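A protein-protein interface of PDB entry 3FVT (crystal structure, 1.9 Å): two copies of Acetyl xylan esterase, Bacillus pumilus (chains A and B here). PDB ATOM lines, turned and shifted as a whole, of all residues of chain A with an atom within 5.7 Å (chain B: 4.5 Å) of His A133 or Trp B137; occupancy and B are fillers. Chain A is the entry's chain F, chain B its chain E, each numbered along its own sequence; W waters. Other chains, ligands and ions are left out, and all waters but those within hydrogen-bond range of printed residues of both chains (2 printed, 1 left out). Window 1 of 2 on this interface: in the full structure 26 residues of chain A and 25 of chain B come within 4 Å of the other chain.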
ATOM      1  N   THR A 129      26.166  -8.510 -28.413  1.00  0.00           N
ATOM      2  CA  THR A 129      25.400  -9.105 -27.324  1.00  0.00           C
ATOM      3  C   THR A 129      25.649  -8.079 -26.228  1.00  0.00           C
ATOM      4  O   THR A 129      26.783  -7.869 -25.826  1.00  0.00           O
ATOM      5  CB  THR A 129      25.947 -10.497 -26.904  1.00  0.00           C
ATOM      6  OG1 THR A 129      25.743 -11.431 -27.972  1.00  0.00           O
ATOM      7  CG2 THR A 129      25.189 -11.017 -25.668  1.00  0.00           C
ATOM      8  N   GLY A 131      24.726  -8.063 -22.982  1.00  0.00           N
ATOM      9  CA  GLY A 131      25.097  -8.606 -21.694  1.00  0.00           C
ATOM     10  C   GLY A 131      24.709 -10.061 -21.560  1.00  0.00           C
ATOM     11  O   GLY A 131      24.450 -10.731 -22.557  1.00  0.00           O
ATOM     12  N   GLY A 132      24.667 -10.556 -20.327  1.00  0.00           N
ATOM     13  CA  GLY A 132      24.319 -11.950 -20.154  1.00  0.00           C
ATOM     14  C   GLY A 132      22.875 -12.278 -20.471  1.00  0.00           C
ATOM     15  O   GLY A 132      21.953 -11.475 -20.237  1.00  0.00           O
ATOM     16  N   HIS A 133      22.685 -13.464 -21.036  1.00  0.00           N
ATOM     17  CA  HIS A 133      21.359 -13.959 -21.361  1.00  0.00           C
ATOM     18  C   HIS A 133      21.362 -15.486 -21.175  1.00  0.00           C
ATOM     19  O   HIS A 133      22.421 -16.087 -20.931  1.00  0.00           O
ATOM     20  CB  HIS A 133      20.965 -13.550 -22.804  1.00  0.00           C
ATOM     21  CG  HIS A 133      21.911 -14.017 -23.874  1.00  0.00           C
ATOM     22  ND1 HIS A 133      21.788 -15.237 -24.498  1.00  0.00           N
ATOM     23  CD2 HIS A 133      22.974 -13.405 -24.453  1.00  0.00           C
ATOM     24  CE1 HIS A 133      22.728 -15.357 -25.420  1.00  0.00           C
ATOM     25  NE2 HIS A 133      23.460 -14.256 -25.413  1.00  0.00           N
ATOM     26  N   ALA A 134      20.189 -16.111 -21.231  1.00  0.00           N
ATOM     27  CA  ALA A 134      20.128 -17.562 -21.071  1.00  0.00           C
ATOM     28  C   ALA A 134      20.463 -18.252 -22.384  1.00  0.00           C
ATOM     29  O   ALA A 134      20.282 -17.691 -23.475  1.00  0.00           O
ATOM     30  CB  ALA A 134      18.739 -18.005 -20.594  1.00  0.00           C
ATOM     31  N   LEU A 135      20.953 -19.483 -22.267  1.00  0.00           N
ATOM     32  CA  LEU A 135      21.312 -20.289 -23.424  1.00  0.00           C
ATOM     33  C   LEU A 135      20.214 -20.116 -24.479  1.00  0.00           C
ATOM     34  O   LEU A 135      19.030 -20.273 -24.171  1.00  0.00           O
ATOM     35  CB  LEU A 135      21.406 -21.757 -22.988  1.00  0.00           C
ATOM     36  CG  LEU A 135      22.265 -22.785 -23.726  1.00  0.00           C
ATOM     37  CD1 LEU A 135      21.879 -24.174 -23.198  1.00  0.00           C
ATOM     38  CD2 LEU A 135      22.064 -22.712 -25.205  1.00  0.00           C
ATOM     39  N   GLY A 136      20.608 -19.776 -25.703  1.00  0.00           N
ATOM     40  CA  GLY A 136      19.652 -19.593 -26.795  1.00  0.00           C
ATOM     41  C   GLY A 136      19.608 -18.170 -27.354  1.00  0.00           C
ATOM     42  O   GLY A 136      20.393 -17.308 -26.956  1.00  0.00           O
ATOM     43  N   TRP A 137      18.693 -17.925 -28.289  1.00  0.00           N
ATOM     44  CA  TRP A 137      18.541 -16.597 -28.888  1.00  0.00           C
ATOM     45  C   TRP A 137      17.383 -15.811 -28.266  1.00  0.00           C
ATOM     46  O   TRP A 137      17.344 -14.590 -28.391  1.00  0.00           O
ATOM     47  CB  TRP A 137      18.277 -16.700 -30.401  1.00  0.00           C
ATOM     48  CG  TRP A 137      19.412 -17.265 -31.213  1.00  0.00           C
ATOM     49  CD1 TRP A 137      20.510 -16.588 -31.688  1.00  0.00           C
ATOM     50  CD2 TRP A 137      19.568 -18.625 -31.634  1.00  0.00           C
ATOM     51  NE1 TRP A 137      21.336 -17.446 -32.387  1.00  0.00           N
ATOM     52  CE2 TRP A 137      20.787 -18.702 -32.365  1.00  0.00           C
ATOM     53  CE3 TRP A 137      18.806 -19.790 -31.464  1.00  0.00           C
ATOM     54  CZ2 TRP A 137      21.253 -19.890 -32.920  1.00  0.00           C
ATOM     55  CZ3 TRP A 137      19.272 -20.978 -32.017  1.00  0.00           C
ATOM     56  CH2 TRP A 137      20.492 -21.018 -32.740  1.00  0.00           C
ATOM     57  N   THR A 139      16.581 -14.635 -25.327  1.00  0.00           N
ATOM     58  CA  THR A 139      16.827 -13.528 -24.416  1.00  0.00           C
ATOM     59  C   THR A 139      18.036 -12.685 -24.797  1.00  0.00           C
ATOM     60  O   THR A 139      18.498 -11.877 -23.985  1.00  0.00           O
ATOM     61  CB  THR A 139      17.003 -14.030 -22.963  1.00  0.00           C
ATOM     62  OG1 THR A 139      18.023 -15.042 -22.914  1.00  0.00           O
ATOM     63  CG2 THR A 139      15.715 -14.602 -22.471  1.00  0.00           C
ATOM     64  N   LYS A 140      18.532 -12.855 -26.027  1.00  0.00           N
ATOM     65  CA  LYS A 140      19.673 -12.067 -26.458  1.00  0.00           C
ATOM     66  C   LYS A 140      19.256 -10.614 -26.685  1.00  0.00           C
ATOM     67  O   LYS A 140      18.486 -10.326 -27.602  1.00  0.00           O
ATOM     68  CB  LYS A 140      20.291 -12.614 -27.749  1.00  0.00           C
ATOM     69  CG  LYS A 140      21.518 -11.807 -28.189  1.00  0.00           C
ATOM     70  CD  LYS A 140      22.154 -12.330 -29.467  1.00  0.00           C
ATOM     71  CE  LYS A 140      23.282 -11.400 -29.899  1.00  0.00           C
ATOM     72  NZ  LYS A 140      23.985 -11.839 -31.134  1.00  0.00           N
ATOM     73  N   GLY A 141      19.792  -9.720 -25.851  1.00  0.00           N
ATOM     74  CA  GLY A 141      19.512  -8.297 -25.955  1.00  0.00           C
ATOM     75  C   GLY A 141      18.132  -7.916 -25.480  1.00  0.00           C
ATOM     76  O   GLY A 141      17.592  -6.863 -25.868  1.00  0.00           O
ATOM     77  N   TYR A 228      16.190 -17.279 -18.074  1.00  0.00           N
ATOM     78  CA  TYR A 228      16.798 -15.958 -17.981  1.00  0.00           C
ATOM     79  C   TYR A 228      16.471 -15.284 -16.639  1.00  0.00           C
ATOM     80  O   TYR A 228      17.366 -14.726 -15.984  1.00  0.00           O
ATOM     81  CB  TYR A 228      16.343 -15.072 -19.163  1.00  0.00           C
ATOM     82  CG  TYR A 228      16.830 -13.641 -19.085  1.00  0.00           C
ATOM     83  CD1 TYR A 228      18.166 -13.306 -19.351  1.00  0.00           C
ATOM     84  CD2 TYR A 228      15.955 -12.611 -18.721  1.00  0.00           C
ATOM     85  CE1 TYR A 228      18.611 -11.968 -19.256  1.00  0.00           C
ATOM     86  CE2 TYR A 228      16.390 -11.280 -18.615  1.00  0.00           C
ATOM     87  CZ  TYR A 228      17.713 -10.966 -18.883  1.00  0.00           C
ATOM     88  OH  TYR A 228      18.129  -9.650 -18.776  1.00  0.00           O
ATOM     89  N   ARG A 231      18.444 -16.652 -13.680  1.00  0.00           N
ATOM     90  CA  ARG A 231      19.838 -16.194 -13.633  1.00  0.00           C
ATOM     91  C   ARG A 231      20.037 -14.704 -13.387  1.00  0.00           C
ATOM     92  O   ARG A 231      21.156 -14.263 -13.120  1.00  0.00           O
ATOM     93  CB  ARG A 231      20.569 -16.556 -14.935  1.00  0.00           C
ATOM     94  CG  ARG A 231      20.854 -18.041 -15.098  1.00  0.00           C
ATOM     95  CD  ARG A 231      20.982 -18.455 -16.572  1.00  0.00           C
ATOM     96  NE  ARG A 231      21.431 -19.843 -16.672  1.00  0.00           N
ATOM     97  CZ  ARG A 231      20.659 -20.906 -16.463  1.00  0.00           C
ATOM     98  NH1 ARG A 231      19.376 -20.753 -16.161  1.00  0.00           N
ATOM     99  NH2 ARG A 231      21.188 -22.123 -16.483  1.00  0.00           N
ATOM    100  N   ASN A 232      18.956 -13.942 -13.478  1.00  0.00           N
ATOM    101  CA  ASN A 232      18.994 -12.498 -13.299  1.00  0.00           C
ATOM    102  C   ASN A 232      17.760 -12.149 -12.508  1.00  0.00           C
ATOM    103  O   ASN A 232      16.757 -11.761 -13.083  1.00  0.00           O
ATOM    104  CB  ASN A 232      18.952 -11.859 -14.677  1.00  0.00           C
ATOM    105  CG  ASN A 232      20.112 -12.296 -15.540  1.00  0.00           C
ATOM    106  OD1 ASN A 232      21.193 -11.716 -15.470  1.00  0.00           O
ATOM    107  ND2 ASN A 232      19.903 -13.354 -16.340  1.00  0.00           N
ATOM    108  N   TYR B  91      29.532 -23.134 -17.814  1.00  0.00           N
ATOM    109  CA  TYR B  91      28.779 -22.835 -19.029  1.00  0.00           C
ATOM    110  C   TYR B  91      27.320 -22.579 -18.670  1.00  0.00           C
ATOM    111  O   TYR B  91      26.661 -23.470 -18.113  1.00  0.00           O
ATOM    112  CB  TYR B  91      28.851 -24.059 -19.946  1.00  0.00           C
ATOM    113  CG  TYR B  91      28.293 -23.837 -21.315  1.00  0.00           C
ATOM    114  CD1 TYR B  91      29.048 -23.194 -22.287  1.00  0.00           C
ATOM    115  CD2 TYR B  91      27.009 -24.292 -21.652  1.00  0.00           C
ATOM    116  CE1 TYR B  91      28.557 -23.007 -23.568  1.00  0.00           C
ATOM    117  CE2 TYR B  91      26.502 -24.106 -22.940  1.00  0.00           C
ATOM    118  CZ  TYR B  91      27.289 -23.463 -23.888  1.00  0.00           C
ATOM    119  OH  TYR B  91      26.817 -23.276 -25.164  1.00  0.00           O
ATOM    120  N   ASN B  92      26.819 -21.382 -18.966  1.00  0.00           N
ATOM    121  CA  ASN B  92      25.407 -21.055 -18.729  1.00  0.00           C
ATOM    122  C   ASN B  92      24.999 -21.320 -17.297  1.00  0.00           C
ATOM    123  O   ASN B  92      23.814 -21.446 -17.005  1.00  0.00           O
ATOM    124  CB  ASN B  92      24.527 -21.911 -19.664  1.00  0.00           C
ATOM    125  CG  ASN B  92      23.060 -21.490 -19.656  1.00  0.00           C
ATOM    126  OD1 ASN B  92      22.744 -20.322 -19.844  1.00  0.00           O
ATOM    127  ND2 ASN B  92      22.156 -22.456 -19.456  1.00  0.00           N
ATOM    128  N   ARG B 118      31.415 -13.686 -21.516  1.00  0.00           N
ATOM    129  CA  ARG B 118      30.669 -13.060 -22.614  1.00  0.00           C
ATOM    130  C   ARG B 118      29.282 -13.593 -22.934  1.00  0.00           C
ATOM    131  O   ARG B 118      29.153 -14.710 -23.412  1.00  0.00           O
ATOM    132  CB  ARG B 118      31.484 -13.153 -23.897  1.00  0.00           C
ATOM    133  CG  ARG B 118      32.800 -12.483 -23.818  1.00  0.00           C
ATOM    134  CD  ARG B 118      33.409 -12.309 -25.210  1.00  0.00           C
ATOM    135  NE  ARG B 118      34.628 -11.520 -25.094  1.00  0.00           N
ATOM    136  CZ  ARG B 118      35.089 -10.687 -26.025  1.00  0.00           C
ATOM    137  NH1 ARG B 118      34.431 -10.518 -27.174  1.00  0.00           N
ATOM    138  NH2 ARG B 118      36.207 -10.007 -25.800  1.00  0.00           N
ATOM    139  N   GLY B 119      28.251 -12.776 -22.709  1.00  0.00           N
ATOM    140  CA  GLY B 119      26.901 -13.215 -23.030  1.00  0.00           C
ATOM    141  C   GLY B 119      26.259 -14.250 -22.121  1.00  0.00           C
ATOM    142  O   GLY B 119      25.053 -14.500 -22.223  1.00  0.00           O
ATOM    143  N   GLN B 120      27.019 -14.854 -21.221  1.00  0.00           N
ATOM    144  CA  GLN B 120      26.413 -15.849 -20.348  1.00  0.00           C
ATOM    145  C   GLN B 120      25.961 -15.236 -19.034  1.00  0.00           C
ATOM    146  O   GLN B 120      24.815 -14.794 -18.912  1.00  0.00           O
ATOM    147  CB  GLN B 120      27.378 -17.006 -20.083  1.00  0.00           C
ATOM    148  CG  GLN B 120      27.642 -17.863 -21.292  1.00  0.00           C
ATOM    149  CD  GLN B 120      28.670 -18.936 -21.014  1.00  0.00           C
ATOM    150  OE1 GLN B 120      28.687 -19.536 -19.927  1.00  0.00           O
ATOM    151  NE2 GLN B 120      29.530 -19.197 -21.991  1.00  0.00           N
ATOM    152  N   GLY B 136      23.232 -22.268 -28.868  1.00  0.00           N
ATOM    153  CA  GLY B 136      24.286 -22.191 -27.881  1.00  0.00           C
ATOM    154  C   GLY B 136      25.523 -21.428 -28.338  1.00  0.00           C
ATOM    155  O   GLY B 136      25.579 -20.870 -29.444  1.00  0.00           O
ATOM    156  N   TRP B 137      26.531 -21.434 -27.474  1.00  0.00           N
ATOM    157  CA  TRP B 137      27.764 -20.710 -27.729  1.00  0.00           C
ATOM    158  C   TRP B 137      28.901 -21.567 -28.271  1.00  0.00           C
ATOM    159  O   TRP B 137      29.858 -21.040 -28.841  1.00  0.00           O
ATOM    160  CB  TRP B 137      28.226 -20.039 -26.425  1.00  0.00           C
ATOM    161  CG  TRP B 137      27.352 -18.894 -25.920  1.00  0.00           C
ATOM    162  CD1 TRP B 137      27.342 -17.607 -26.366  1.00  0.00           C
ATOM    163  CD2 TRP B 137      26.432 -18.942 -24.819  1.00  0.00           C
ATOM    164  NE1 TRP B 137      26.478 -16.841 -25.607  1.00  0.00           N
ATOM    165  CE2 TRP B 137      25.905 -17.640 -24.652  1.00  0.00           C
ATOM    166  CE3 TRP B 137      26.003 -19.959 -23.961  1.00  0.00           C
ATOM    167  CZ2 TRP B 137      24.967 -17.327 -23.655  1.00  0.00           C
ATOM    168  CZ3 TRP B 137      25.061 -19.649 -22.961  1.00  0.00           C
ATOM    169  CH2 TRP B 137      24.557 -18.337 -22.824  1.00  0.00           C
ATOM    170  N   MET B 138      28.787 -22.883 -28.116  1.00  0.00           N
ATOM    171  CA  MET B 138      29.851 -23.785 -28.535  1.00  0.00           C
ATOM    172  C   MET B 138      30.265 -23.692 -29.981  1.00  0.00           C
ATOM    173  O   MET B 138      31.442 -23.871 -30.292  1.00  0.00           O
ATOM    174  CB  MET B 138      29.480 -25.233 -28.221  1.00  0.00           C
ATOM    175  CG  MET B 138      29.423 -25.530 -26.738  1.00  0.00           C
ATOM    176  SD  MET B 138      31.018 -25.234 -25.934  1.00  0.00           S
ATOM    177  CE  MET B 138      32.114 -26.436 -26.749  1.00  0.00           C
ATOM    178  N   THR B 139      29.313 -23.416 -30.869  1.00  0.00           N
ATOM    179  CA  THR B 139      29.649 -23.339 -32.270  1.00  0.00           C
ATOM    180  C   THR B 139      29.532 -21.954 -32.917  1.00  0.00           C
ATOM    181  O   THR B 139      29.547 -21.833 -34.135  1.00  0.00           O
ATOM    182  CB  THR B 139      28.829 -24.388 -33.083  1.00  0.00           C
ATOM    183  OG1 THR B 139      27.434 -24.130 -32.943  1.00  0.00           O
ATOM    184  CG2 THR B 139      29.103 -25.795 -32.565  1.00  0.00           C
ATOM    185  N   LYS B 140      29.405 -20.906 -32.111  1.00  0.00           N
ATOM    186  CA  LYS B 140      29.358 -19.554 -32.662  1.00  0.00           C
ATOM    187  C   LYS B 140      30.728 -19.213 -33.267  1.00  0.00           C
ATOM    188  O   LYS B 140      31.761 -19.263 -32.580  1.00  0.00           O
ATOM    189  CB  LYS B 140      29.021 -18.519 -31.583  1.00  0.00           C
ATOM    190  CG  LYS B 140      29.209 -17.058 -32.049  1.00  0.00           C
ATOM    191  CD  LYS B 140      28.785 -16.063 -30.960  1.00  0.00           C
ATOM    192  CE  LYS B 140      29.054 -14.603 -31.372  1.00  0.00           C
ATOM    193  NZ  LYS B 140      28.812 -13.654 -30.246  1.00  0.00           N
ATOM    194  N   TYR B 149      33.914 -18.120 -30.689  1.00  0.00           N
ATOM    195  CA  TYR B 149      33.473 -17.630 -29.391  1.00  0.00           C
ATOM    196  C   TYR B 149      34.525 -17.629 -28.288  1.00  0.00           C
ATOM    197  O   TYR B 149      34.677 -16.632 -27.588  1.00  0.00           O
ATOM    198  CB  TYR B 149      32.275 -18.451 -28.913  1.00  0.00           C
ATOM    199  CG  TYR B 149      31.772 -18.057 -27.543  1.00  0.00           C
ATOM    200  CD1 TYR B 149      31.062 -16.869 -27.357  1.00  0.00           C
ATOM    201  CD2 TYR B 149      32.002 -18.868 -26.438  1.00  0.00           C
ATOM    202  CE1 TYR B 149      30.592 -16.497 -26.105  1.00  0.00           C
ATOM    203  CE2 TYR B 149      31.530 -18.501 -25.164  1.00  0.00           C
ATOM    204  CZ  TYR B 149      30.827 -17.310 -25.013  1.00  0.00           C
ATOM    205  OH  TYR B 149      30.371 -16.943 -23.760  1.00  0.00           O
ATOM    206  N   GLU B 224      26.673 -29.926 -28.613  1.00  0.00           N
ATOM    207  CA  GLU B 224      26.229 -28.808 -29.448  1.00  0.00           C
ATOM    208  C   GLU B 224      27.019 -28.934 -30.766  1.00  0.00           C
ATOM    209  O   GLU B 224      26.547 -28.560 -31.845  1.00  0.00           O
ATOM    210  CB  GLU B 224      26.545 -27.468 -28.762  1.00  0.00           C
ATOM    211  CG  GLU B 224      25.509 -27.026 -27.720  1.00  0.00           C
ATOM    212  CD  GLU B 224      25.802 -25.654 -27.154  1.00  0.00           C
ATOM    213  OE1 GLU B 224      26.452 -24.858 -27.868  1.00  0.00           O
ATOM    214  OE2 GLU B 224      25.361 -25.351 -26.020  1.00  0.00           O
HETATM  215  O   HOH W   1      25.504 -14.429 -27.306  1.00  0.00           O
HETATM  216  O   HOH W   2      27.297 -11.089 -30.200  1.00  0.00           O
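Of chain B, only Gly B119 (2.8 Å), Gln B120 (3.3 Å) and Trp B137 (3.5 Å) come within 4 Å of His A133. Of the printed residues of chain A, Trp B137 touches His A133 (3.5 Å) and Leu A135 (3.8 Å). Printed residues of chain B within 4 Å of Gly A132: Gly B119 (3.4 Å) and Gln B120 (3.1 Å). Of the printed residues of chain B, Leu A135 touches Asn B92 (3.1 Å), Gly B136 (3.5 Å) and Trp B137 (3.8 Å). Printed residues of chain B within 4 Å of Gly A131: Gly B119 (3.5 Å). Of the printed residues of chain A, Asn B92 touches Ala A134 (3.99 Å), Leu A135 (3.1 Å) and Arg A231 (2.8 Å). Of the printed residues of chain B, Thr A129 touches Gly B119. Gly A136 touches none of the printed residues of chain B. Trp A137 touches none of the printed residues of chain B. The nearest residue of chain B that does not touch His A133 is Asn B92 (4.4 Å). The nearest printed residue of chain B that does not touch Arg A231 is Gln B120 (5.8 Å).
4 positions are printed for both chains.
Water W2 bridges the side-chain hydroxyl of Thr A129 (2.7 Å) and the side-chain amino group of Lys B140 (3.0 Å). Water W1 lies within hydrogen-bond range of a ring nitrogen (NE2) of His A133 (2.8 Å), the side-chain hydroxyl of Thr A129 (3.1 Å) and the indole nitrogen of Trp B137 (3.1 Å).
Thr A129 touches Gly B119 (CG2 to CA, 3.8 Å). Gly B119 touches Gly A131 (CA to O, 3.5 Å). Gly A132 touches Gly B119. O of Gln B120 touches CA of Gly A132 (3.1 Å). CZ2 of Trp B137 touches CE1 of His A133 (3.5 Å). Ala A134 touches Asn B92 (C to OD1, 3.99 Å). CD2 of Leu A135 touches CA of Gly B136, 3.5 Å away. Leu A135 touches Trp B137.
Of the 14 printed residues of chain A, 7 touch a printed residue of chain B. Hydrophobic or aromatic side chains of chain A within 4 Å of the printed part of chain B: His A133 and Leu A135. Hydrophobic or aromatic side chains of chain B within 4 Å of the printed part of chain A: Trp B137.
OD1 of Asn B92 lies within hydrogen-bond range of N of Leu A135 (3.1 Å). O of Asn B92 is in hydrogen-bond range of NH2 of Arg A231 (2.8 Å). O of Gly B119 is in hydrogen-bond range of N of His A133 (2.8 Å). The backbone carbonyl oxygen of Gln B120 sits at hydrogen-bond distance from the backbone NH of His A133 (3.3 Å).
The backbone NH (N) of Trp B137 is in hydrogen-bond range of the side-chain hydroxyl (OH) of Tyr B91, at 3.0 Å. N of Asn B92 sits at hydrogen-bond distance from OE1 of Gln B120. The side-chain amide nitrogen of Gln B120 lies within hydrogen-bond range of the side-chain hydroxyl of Tyr B149 (3.0 Å). The backbone NH (N) of Trp B137 sits at hydrogen-bond distance from the side-chain carboxylate (OE1) of Glu B224 (3.4 Å). N of Ala A134 lies within hydrogen-bond range of OG1 of Thr A139.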
